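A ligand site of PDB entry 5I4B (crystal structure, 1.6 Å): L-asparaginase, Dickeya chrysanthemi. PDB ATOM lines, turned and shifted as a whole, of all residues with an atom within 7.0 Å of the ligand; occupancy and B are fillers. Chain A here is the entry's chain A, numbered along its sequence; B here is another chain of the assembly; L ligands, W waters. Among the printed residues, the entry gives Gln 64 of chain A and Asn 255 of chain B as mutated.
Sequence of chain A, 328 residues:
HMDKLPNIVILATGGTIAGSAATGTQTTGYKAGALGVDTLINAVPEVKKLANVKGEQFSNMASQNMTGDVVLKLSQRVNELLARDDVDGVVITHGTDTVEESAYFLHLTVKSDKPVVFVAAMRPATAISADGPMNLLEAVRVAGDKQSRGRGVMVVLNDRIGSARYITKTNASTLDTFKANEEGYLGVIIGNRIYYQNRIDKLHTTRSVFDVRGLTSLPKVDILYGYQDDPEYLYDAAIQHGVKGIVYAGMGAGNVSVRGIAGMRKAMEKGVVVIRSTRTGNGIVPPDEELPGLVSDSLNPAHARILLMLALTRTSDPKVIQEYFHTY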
ATOM      1  N   GLY A  14      18.715 -17.977 -23.718  1.00  0.00           N
ATOM      2  CA  GLY A  14      17.782 -17.235 -22.843  1.00  0.00           C
ATOM      3  C   GLY A  14      17.091 -18.070 -21.776  1.00  0.00           C
ATOM      4  O   GLY A  14      17.670 -19.000 -21.193  1.00  0.00           O
ATOM      5  N   GLY A  15      15.873 -17.682 -21.431  1.00  0.00           N
ATOM      6  CA  GLY A  15      15.103 -18.385 -20.359  1.00  0.00           C
ATOM      7  C   GLY A  15      15.156 -17.811 -18.936  1.00  0.00           C
ATOM      8  O   GLY A  15      16.030 -17.017 -18.619  1.00  0.00           O
ATOM      9  N   THR A  16      14.290 -18.321 -18.046  1.00  0.00           N
ATOM     10  CA  THR A  16      14.332 -17.957 -16.612  1.00  0.00           C
ATOM     11  C   THR A  16      15.682 -18.324 -15.976  1.00  0.00           C
ATOM     12  O   THR A  16      16.168 -17.664 -15.026  1.00  0.00           O
ATOM     13  CB  THR A  16      13.153 -18.625 -15.876  1.00  0.00           C
ATOM     14  OG1 THR A  16      11.968 -18.009 -16.381  1.00  0.00           O
ATOM     15  CG2 THR A  16      13.209 -18.530 -14.381  1.00  0.00           C
ATOM     16  N   ILE A  17      16.367 -19.338 -16.542  1.00  0.00           N
ATOM     17  CA  ILE A  17      17.753 -19.665 -16.054  1.00  0.00           C
ATOM     18  C   ILE A  17      18.723 -18.496 -16.085  1.00  0.00           C
ATOM     19  O   ILE A  17      19.687 -18.459 -15.308  1.00  0.00           O
ATOM     20  CB  ILE A  17      18.348 -20.887 -16.790  1.00  0.00           C
ATOM     21  CG1 ILE A  17      19.580 -21.413 -16.083  1.00  0.00           C
ATOM     22  CG2 ILE A  17      18.567 -20.569 -18.288  1.00  0.00           C
ATOM     23  CD1 ILE A  17      19.945 -22.837 -16.584  1.00  0.00           C
ATOM     24  N   ALA A  18      18.485 -17.579 -17.033  1.00  0.00           N
ATOM     25  CA  ALA A  18      19.267 -16.336 -17.154  1.00  0.00           C
ATOM     26  C   ALA A  18      18.389 -15.114 -16.756  1.00  0.00           C
ATOM     27  O   ALA A  18      18.650 -13.943 -17.184  1.00  0.00           O
ATOM     28  CB  ALA A  18      19.748 -16.195 -18.624  1.00  0.00           C
ATOM     29  N   TYR A  30       9.734 -10.223 -14.463  1.00  0.00           N
ATOM     30  CA  TYR A  30      11.217 -10.058 -14.624  1.00  0.00           C
ATOM     31  C   TYR A  30      11.519 -10.475 -16.103  1.00  0.00           C
ATOM     32  O   TYR A  30      10.725 -11.210 -16.694  1.00  0.00           O
ATOM     33  CB  TYR A  30      12.051 -10.881 -13.576  1.00  0.00           C
ATOM     34  CG  TYR A  30      11.814 -12.380 -13.697  1.00  0.00           C
ATOM     35  CD1 TYR A  30      12.531 -13.134 -14.638  1.00  0.00           C
ATOM     36  CD2 TYR A  30      10.818 -13.014 -12.947  1.00  0.00           C
ATOM     37  CE1 TYR A  30      12.262 -14.491 -14.820  1.00  0.00           C
ATOM     38  CE2 TYR A  30      10.546 -14.362 -13.107  1.00  0.00           C
ATOM     39  CZ  TYR A  30      11.270 -15.098 -14.036  1.00  0.00           C
ATOM     40  OH  TYR A  30      11.015 -16.441 -14.213  1.00  0.00           O
ATOM     41  N   ALA A  32      13.154 -12.720 -18.657  1.00  0.00           N
ATOM     42  CA  ALA A  32      13.806 -14.005 -18.857  1.00  0.00           C
ATOM     43  C   ALA A  32      14.900 -13.699 -19.932  1.00  0.00           C
ATOM     44  O   ALA A  32      14.715 -12.873 -20.812  1.00  0.00           O
ATOM     45  CB  ALA A  32      12.788 -15.091 -19.254  1.00  0.00           C
ATOM     46  N   GLY A  33      16.088 -14.238 -19.746  1.00  0.00           N
ATOM     47  CA  GLY A  33      17.174 -14.009 -20.716  1.00  0.00           C
ATOM     48  C   GLY A  33      17.744 -12.600 -20.595  1.00  0.00           C
ATOM     49  O   GLY A  33      17.866 -11.903 -21.607  1.00  0.00           O
ATOM     50  N   MET A  61      16.485 -14.707 -25.337  1.00  0.00           N
ATOM     51  CA  MET A  61      15.065 -14.485 -25.325  1.00  0.00           C
ATOM     52  C   MET A  61      14.333 -15.406 -24.378  1.00  0.00           C
ATOM     53  O   MET A  61      14.833 -16.477 -24.012  1.00  0.00           O
ATOM     54  CB  MET A  61      14.578 -14.670 -26.746  1.00  0.00           C
ATOM     55  CG  MET A  61      14.545 -16.093 -27.194  1.00  0.00           C
ATOM     56  SD  MET A  61      13.833 -16.273 -28.812  1.00  0.00           S
ATOM     57  CE  MET A  61      15.231 -15.913 -29.852  1.00  0.00           C
ATOM     58  N   ALA A  62      13.118 -15.015 -24.046  1.00  0.00           N
ATOM     59  CA  ALA A  62      12.210 -15.899 -23.279  1.00  0.00           C
ATOM     60  C   ALA A  62      11.686 -16.941 -24.264  1.00  0.00           C
ATOM     61  O   ALA A  62      11.398 -16.632 -25.452  1.00  0.00           O
ATOM     62  CB  ALA A  62      11.098 -15.055 -22.664  1.00  0.00           C
ATOM     63  N   SER A  63      11.608 -18.231 -23.835  1.00  0.00           N
ATOM     64  CA  SER A  63      11.337 -19.290 -24.809  1.00  0.00           C
ATOM     65  C   SER A  63       9.973 -19.269 -25.379  1.00  0.00           C
ATOM     66  O   SER A  63       9.719 -19.883 -26.462  1.00  0.00           O
ATOM     67  CB  SER A  63      11.660 -20.648 -24.271  1.00  0.00           C
ATOM     68  OG  SER A  63      10.653 -21.118 -23.397  1.00  0.00           O
ATOM     69  N   GLN A  64       9.020 -18.555 -24.749  1.00  0.00           N
ATOM     70  CA  GLN A  64       7.721 -18.397 -25.386  1.00  0.00           C
ATOM     71  C   GLN A  64       7.824 -17.637 -26.732  1.00  0.00           C
ATOM     72  O   GLN A  64       6.900 -17.653 -27.512  1.00  0.00           O
ATOM     73  CB  GLN A  64       6.677 -17.721 -24.475  1.00  0.00           C
ATOM     74  CG  GLN A  64       6.993 -16.307 -24.036  1.00  0.00           C
ATOM     75  CD  GLN A  64       7.850 -16.179 -22.823  1.00  0.00           C
ATOM     76  OE1 GLN A  64       8.702 -17.029 -22.526  1.00  0.00           O
ATOM     77  NE2 GLN A  64       7.637 -15.105 -22.060  1.00  0.00           N
ATOM     78  N   ASN A  65       8.910 -16.909 -26.915  1.00  0.00           N
ATOM     79  CA  ASN A  65       9.205 -16.227 -28.164  1.00  0.00           C
ATOM     80  C   ASN A  65      10.153 -16.913 -29.109  1.00  0.00           C
ATOM     81  O   ASN A  65      10.415 -16.414 -30.179  1.00  0.00           O
ATOM     82  CB  ASN A  65       9.696 -14.826 -27.866  1.00  0.00           C
ATOM     83  CG  ASN A  65       8.570 -13.941 -27.470  1.00  0.00           C
ATOM     84  OD1 ASN A  65       7.578 -13.884 -28.160  1.00  0.00           O
ATOM     85  ND2 ASN A  65       8.697 -13.329 -26.362  1.00  0.00           N
ATOM     86  N   HIS A  94      18.062 -22.666 -21.963  1.00  0.00           N
ATOM     87  CA  HIS A  94      16.839 -22.332 -22.681  1.00  0.00           C
ATOM     88  C   HIS A  94      15.735 -22.074 -21.661  1.00  0.00           C
ATOM     89  O   HIS A  94      15.796 -22.575 -20.530  1.00  0.00           O
ATOM     90  CB  HIS A  94      16.493 -23.540 -23.607  1.00  0.00           C
ATOM     91  CG  HIS A  94      15.524 -23.336 -24.691  1.00  0.00           C
ATOM     92  ND1 HIS A  94      14.155 -23.324 -24.490  1.00  0.00           N
ATOM     93  CD2 HIS A  94      15.687 -23.289 -26.058  1.00  0.00           C
ATOM     94  CE1 HIS A  94      13.522 -23.284 -25.650  1.00  0.00           C
ATOM     95  NE2 HIS A  94      14.443 -23.217 -26.612  1.00  0.00           N
ATOM     96  N   GLY A  95      14.720 -21.347 -22.055  1.00  0.00           N
ATOM     97  CA  GLY A  95      13.558 -21.217 -21.223  1.00  0.00           C
ATOM     98  C   GLY A  95      12.803 -22.527 -21.141  1.00  0.00           C
ATOM     99  O   GLY A  95      12.836 -23.398 -22.054  1.00  0.00           O
ATOM    100  N   THR A  96      12.082 -22.739 -20.045  1.00  0.00           N
ATOM    101  CA  THR A  96      11.330 -23.976 -19.864  1.00  0.00           C
ATOM    102  C   THR A  96      10.096 -24.128 -20.713  1.00  0.00           C
ATOM    103  O   THR A  96       9.714 -25.234 -21.037  1.00  0.00           O
ATOM    104  CB  THR A  96      10.885 -24.159 -18.376  1.00  0.00           C
ATOM    105  OG1 THR A  96      10.010 -23.090 -18.036  1.00  0.00           O
ATOM    106  CG2 THR A  96      11.980 -24.225 -17.439  1.00  0.00           C
ATOM    107  N   ASP A  97       9.446 -23.007 -21.096  1.00  0.00           N
ATOM    108  CA  ASP A  97       8.146 -23.069 -21.721  1.00  0.00           C
ATOM    109  C   ASP A  97       8.098 -23.846 -23.040  1.00  0.00           C
ATOM    110  O   ASP A  97       7.163 -24.549 -23.256  1.00  0.00           O
ATOM    111  CB  ASP A  97       7.583 -21.633 -21.941  1.00  0.00           C
ATOM    112  CG  ASP A  97       7.285 -20.921 -20.633  1.00  0.00           C
ATOM    113  OD1 ASP A  97       7.226 -21.559 -19.560  1.00  0.00           O
ATOM    114  OD2 ASP A  97       7.083 -19.680 -20.692  1.00  0.00           O
ATOM    115  N   THR A  98       9.109 -23.648 -23.893  1.00  0.00           N
ATOM    116  CA  THR A  98       9.157 -24.338 -25.196  1.00  0.00           C
ATOM    117  C   THR A  98      10.418 -25.203 -25.348  1.00  0.00           C
ATOM    118  O   THR A  98      10.712 -25.629 -26.491  1.00  0.00           O
ATOM    119  CB  THR A  98       8.912 -23.383 -26.368  1.00  0.00           C
ATOM    120  OG1 THR A  98      10.095 -22.594 -26.503  1.00  0.00           O
ATOM    121  CG2 THR A  98       7.644 -22.590 -26.162  1.00  0.00           C
ATOM    122  N   VAL A  99      11.177 -25.465 -24.261  1.00  0.00           N
ATOM    123  CA  VAL A  99      12.347 -26.345 -24.372  1.00  0.00           C
ATOM    124  C   VAL A  99      12.037 -27.677 -25.034  1.00  0.00           C
ATOM    125  O   VAL A  99      12.877 -28.208 -25.778  1.00  0.00           O
ATOM    126  CB  VAL A  99      13.094 -26.522 -23.032  1.00  0.00           C
ATOM    127  CG1 VAL A  99      12.351 -27.400 -22.060  1.00  0.00           C
ATOM    128  CG2 VAL A  99      14.527 -27.037 -23.289  1.00  0.00           C
ATOM    129  N   ALA A 120      17.428 -25.861 -18.213  1.00  0.00           N
ATOM    130  CA  ALA A 120      16.545 -24.713 -17.982  1.00  0.00           C
ATOM    131  C   ALA A 120      16.344 -24.610 -16.463  1.00  0.00           C
ATOM    132  O   ALA A 120      16.904 -25.425 -15.683  1.00  0.00           O
ATOM    133  CB  ALA A 120      15.232 -24.909 -18.710  1.00  0.00           C
ATOM    134  N   ALA A 121      15.618 -23.584 -16.046  1.00  0.00           N
ATOM    135  CA  ALA A 121      15.356 -23.343 -14.619  1.00  0.00           C
ATOM    136  C   ALA A 121      13.950 -22.794 -14.483  1.00  0.00           C
ATOM    137  O   ALA A 121      13.494 -21.935 -15.260  1.00  0.00           O
ATOM    138  CB  ALA A 121      16.360 -22.405 -13.997  1.00  0.00           C
ATOM    139  N   MET A 122      13.219 -23.328 -13.495  1.00  0.00           N
ATOM    140  CA  MET A 122      11.878 -22.844 -13.168  1.00  0.00           C
ATOM    141  C   MET A 122      11.891 -21.590 -12.277  1.00  0.00           C
ATOM    142  O   MET A 122      10.869 -20.818 -12.290  1.00  0.00           O
ATOM    143  CB  MET A 122      11.045 -23.956 -12.591  1.00  0.00           C
ATOM    144  CG  MET A 122      10.625 -24.982 -13.650  1.00  0.00           C
ATOM    145  SD  MET A 122       9.449 -24.365 -14.839  1.00  0.00           S
ATOM    146  CE  MET A 122       7.951 -24.314 -13.869  1.00  0.00           C
ATOM    147  N   ARG A 123      12.958 -21.321 -11.572  1.00  0.00           N
ATOM    148  CA  ARG A 123      13.085 -20.114 -10.769  1.00  0.00           C
ATOM    149  C   ARG A 123      14.186 -19.246 -11.348  1.00  0.00           C
ATOM    150  O   ARG A 123      15.200 -19.788 -11.865  1.00  0.00           O
ATOM    151  CB  ARG A 123      13.429 -20.467  -9.315  1.00  0.00           C
ATOM    152  CG  ARG A 123      12.300 -21.155  -8.577  1.00  0.00           C
ATOM    153  CD  ARG A 123      12.739 -21.606  -7.216  1.00  0.00           C
ATOM    154  NE  ARG A 123      11.663 -22.337  -6.537  1.00  0.00           N
ATOM    155  CZ  ARG A 123      11.843 -23.106  -5.458  1.00  0.00           C
ATOM    156  NH1 ARG A 123      13.032 -23.334  -4.925  1.00  0.00           N
ATOM    157  NH2 ARG A 123      10.780 -23.669  -4.906  1.00  0.00           N
ATOM    158  N   PRO A 124      14.046 -17.919 -11.297  1.00  0.00           N
ATOM    159  CA  PRO A 124      15.147 -17.089 -11.852  1.00  0.00           C
ATOM    160  C   PRO A 124      16.401 -17.164 -11.060  1.00  0.00           C
ATOM    161  O   PRO A 124      16.372 -17.553  -9.922  1.00  0.00           O
ATOM    162  CB  PRO A 124      14.572 -15.671 -11.849  1.00  0.00           C
ATOM    163  CG  PRO A 124      13.522 -15.702 -10.776  1.00  0.00           C
ATOM    164  CD  PRO A 124      12.905 -17.120 -10.829  1.00  0.00           C
ATOM    165  N   LYS A 169       6.933 -30.447 -20.261  1.00  0.00           N
ATOM    166  CA  LYS A 169       6.570 -29.638 -19.118  1.00  0.00           C
ATOM    167  C   LYS A 169       5.154 -29.960 -18.719  1.00  0.00           C
ATOM    168  O   LYS A 169       4.181 -29.671 -19.459  1.00  0.00           O
ATOM    169  CB  LYS A 169       6.720 -28.166 -19.524  1.00  0.00           C
ATOM    170  CG  LYS A 169       6.594 -27.235 -18.317  1.00  0.00           C
ATOM    171  CD  LYS A 169       6.963 -25.768 -18.661  1.00  0.00           C
ATOM    172  CE  LYS A 169       6.823 -24.874 -17.396  1.00  0.00           C
ATOM    173  NZ  LYS A 169       7.409 -23.525 -17.605  1.00  0.00           N
ATOM    174  N   ALA A 172       2.550 -26.051 -14.864  1.00  0.00           N
ATOM    175  CA  ALA A 172       2.844 -24.660 -15.127  1.00  0.00           C
ATOM    176  C   ALA A 172       4.005 -24.062 -14.388  1.00  0.00           C
ATOM    177  O   ALA A 172       4.716 -23.208 -14.929  1.00  0.00           O
ATOM    178  CB  ALA A 172       1.605 -23.827 -14.834  1.00  0.00           C
ATOM    179  N   MET B 251       1.763 -21.647 -23.107  1.00  0.00           N
ATOM    180  CA  MET B 251       3.088 -22.159 -22.919  1.00  0.00           C
ATOM    181  C   MET B 251       3.459 -21.954 -21.445  1.00  0.00           C
ATOM    182  O   MET B 251       3.318 -20.863 -20.904  1.00  0.00           O
ATOM    183  CB  MET B 251       4.113 -21.486 -23.841  1.00  0.00           C
ATOM    184  CG  MET B 251       3.838 -21.796 -25.320  1.00  0.00           C
ATOM    185  SD  MET B 251       4.834 -20.795 -26.453  1.00  0.00           S
ATOM    186  CE  MET B 251       3.807 -19.335 -26.627  1.00  0.00           C
ATOM    187  N   GLY B 252       3.878 -23.030 -20.761  1.00  0.00           N
ATOM    188  CA  GLY B 252       4.173 -22.920 -19.371  1.00  0.00           C
ATOM    189  C   GLY B 252       3.039 -22.331 -18.533  1.00  0.00           C
ATOM    190  O   GLY B 252       1.889 -22.721 -18.686  1.00  0.00           O
ATOM    191  N   ALA B 253       3.369 -21.328 -17.780  1.00  0.00           N
ATOM    192  CA  ALA B 253       2.448 -20.697 -16.836  1.00  0.00           C
ATOM    193  C   ALA B 253       1.686 -19.584 -17.545  1.00  0.00           C
ATOM    194  O   ALA B 253       1.801 -18.417 -17.163  1.00  0.00           O
ATOM    195  CB  ALA B 253       3.214 -20.171 -15.642  1.00  0.00           C
ATOM    196  N   ASN B 255       2.179 -18.337 -20.394  1.00  0.00           N
ATOM    197  CA  ASN B 255       2.979 -17.329 -21.068  1.00  0.00           C
ATOM    198  C   ASN B 255       2.687 -17.235 -22.538  1.00  0.00           C
ATOM    199  O   ASN B 255       2.206 -18.184 -23.167  1.00  0.00           O
ATOM    200  CB  ASN B 255       4.445 -17.617 -20.841  1.00  0.00           C
ATOM    201  CG  ASN B 255       4.934 -16.987 -19.563  1.00  0.00           C
ATOM    202  OD1 ASN B 255       4.613 -15.812 -19.271  1.00  0.00           O
ATOM    203  ND2 ASN B 255       5.687 -17.757 -18.749  1.00  0.00           N
HETATM  204  N1  LIG L   1       9.017 -17.966 -19.696  1.00  0.00           N
HETATM  205  C1  LIG L   1      10.289 -18.550 -19.230  1.00  0.00           C
HETATM  206  C2  LIG L   1      10.897 -19.058 -20.495  1.00  0.00           C
HETATM  207  O1  LIG L   1      10.414 -20.084 -20.995  1.00  0.00           O
HETATM  208  C3  LIG L   1       9.921 -19.671 -18.225  1.00  0.00           C
HETATM  209  C4  LIG L   1      11.114 -20.439 -17.724  1.00  0.00           C
HETATM  210  O2  LIG L   1      10.905 -21.053 -16.635  1.00  0.00           O
HETATM  211  O3  LIG L   1      12.225 -20.355 -18.347  1.00  0.00           O
HETATM  212  O4  LIG L   1      11.782 -18.380 -21.120  1.00  0.00           O
HETATM  213  O   HOH W   1       9.019 -14.835 -19.519  1.00  0.00           O
HETATM  214  O   HOH W   2       9.336 -20.417 -14.737  1.00  0.00           O
HETATM  215  O   HOH W   3       8.261 -16.433 -17.371  1.00  0.00           O
HETATM  216  O   HOH W   4      15.072 -21.513 -18.043  1.00  0.00           O
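The backbone NH (N) of Thr 96 sits at hydrogen-bond distance from an oxygen (O3) of the ligand (2.9 Å).
N1 of the ligand sits close to ND2 of Asn 255 of chain B, 3.5 Å away.
The side-chain amide oxygen of Gln 64 is in hydrogen-bond range of a nitrogen (N1) of the ligand.
The backbone NH of Thr 16 sits at hydrogen-bond distance from an oxygen (O3) of the ligand, 2.9 Å away.
O4 of the ligand is in hydrogen-bond range of N of Ser 63.
The side-chain hydroxyl of Thr 16 sits close to an oxygen (O3) of the ligand (3.1 Å).
The side-chain hydroxyl (OG1) of Thr 96 lies within hydrogen-bond range of an oxygen (O2) of the ligand, at 2.6 Å.
The side-chain hydroxyl (OG) of Ser 63 lies within hydrogen-bond range of an oxygen (O1) of the ligand (2.6 Å).
O of Ala 121 sits close to O2 of the ligand (3.1 Å).
The side-chain carboxylate of Asp 97 lies within salt-bridge range of a nitrogen (N1) of the ligand.
The backbone NH (N) of Asp 97 is in hydrogen-bond range of an oxygen (O1) of the ligand, 3.1 Å away.
SD of Met 122 is in hydrogen-bond range of OG1 of Thr 96 (3.5 Å).
The backbone NH (N) of Asp 97 sits at hydrogen-bond distance from the side-chain hydroxyl (OG) of Ser 63 (3.2 Å).
OH of Tyr 30 sits at hydrogen-bond distance from OG1 of Thr 16 (2.8 Å).
The side-chain hydroxyl of Thr 96 sits at hydrogen-bond distance from the side-chain amino group of Lys 169 (2.7 Å).
OD2 of Asp 97 is in hydrogen-bond range of ND2 of Asn 255 of chain B (3.1 Å).
The side-chain carboxylate (OD1) of Asp 97 is in salt-bridge range of the side-chain amino group (NZ) of Lys 169, at 2.8 Å.
The backbone carbonyl oxygen (O) of Gly 95 sits close to the side-chain hydroxyl (OG) of Ser 63, 3.4 Å away.
The backbone NH of Gly 33 sits at hydrogen-bond distance from the backbone carbonyl oxygen of Gly 15, 3.0 Å away.
Gly 15 touches the ligand.
CB of Ala 32 touches O4 of the ligand, 3.9 Å away.
Ala 62 touches the ligand.
CA of Gly 95 touches O3 of the ligand, 3.3 Å away.
Hydrophobic or aromatic side chains within 4 Å of the ligand: Ala 32 and Ala 62.
Of the 30 residues printed, 11 come within 4 Å of the ligand.
Water W2 bridges O2 of the ligand (2.5 Å) and O of Met 122 (2.9 Å).
Water W3 lies within hydrogen-bond range of N1 of the ligand (2.9 Å) and ND2 of Asn 255 of chain B (3.2 Å).
Water W1 bridges NE2 of Gln 64 (2.9 Å) and N1 of the ligand (3.1 Å).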
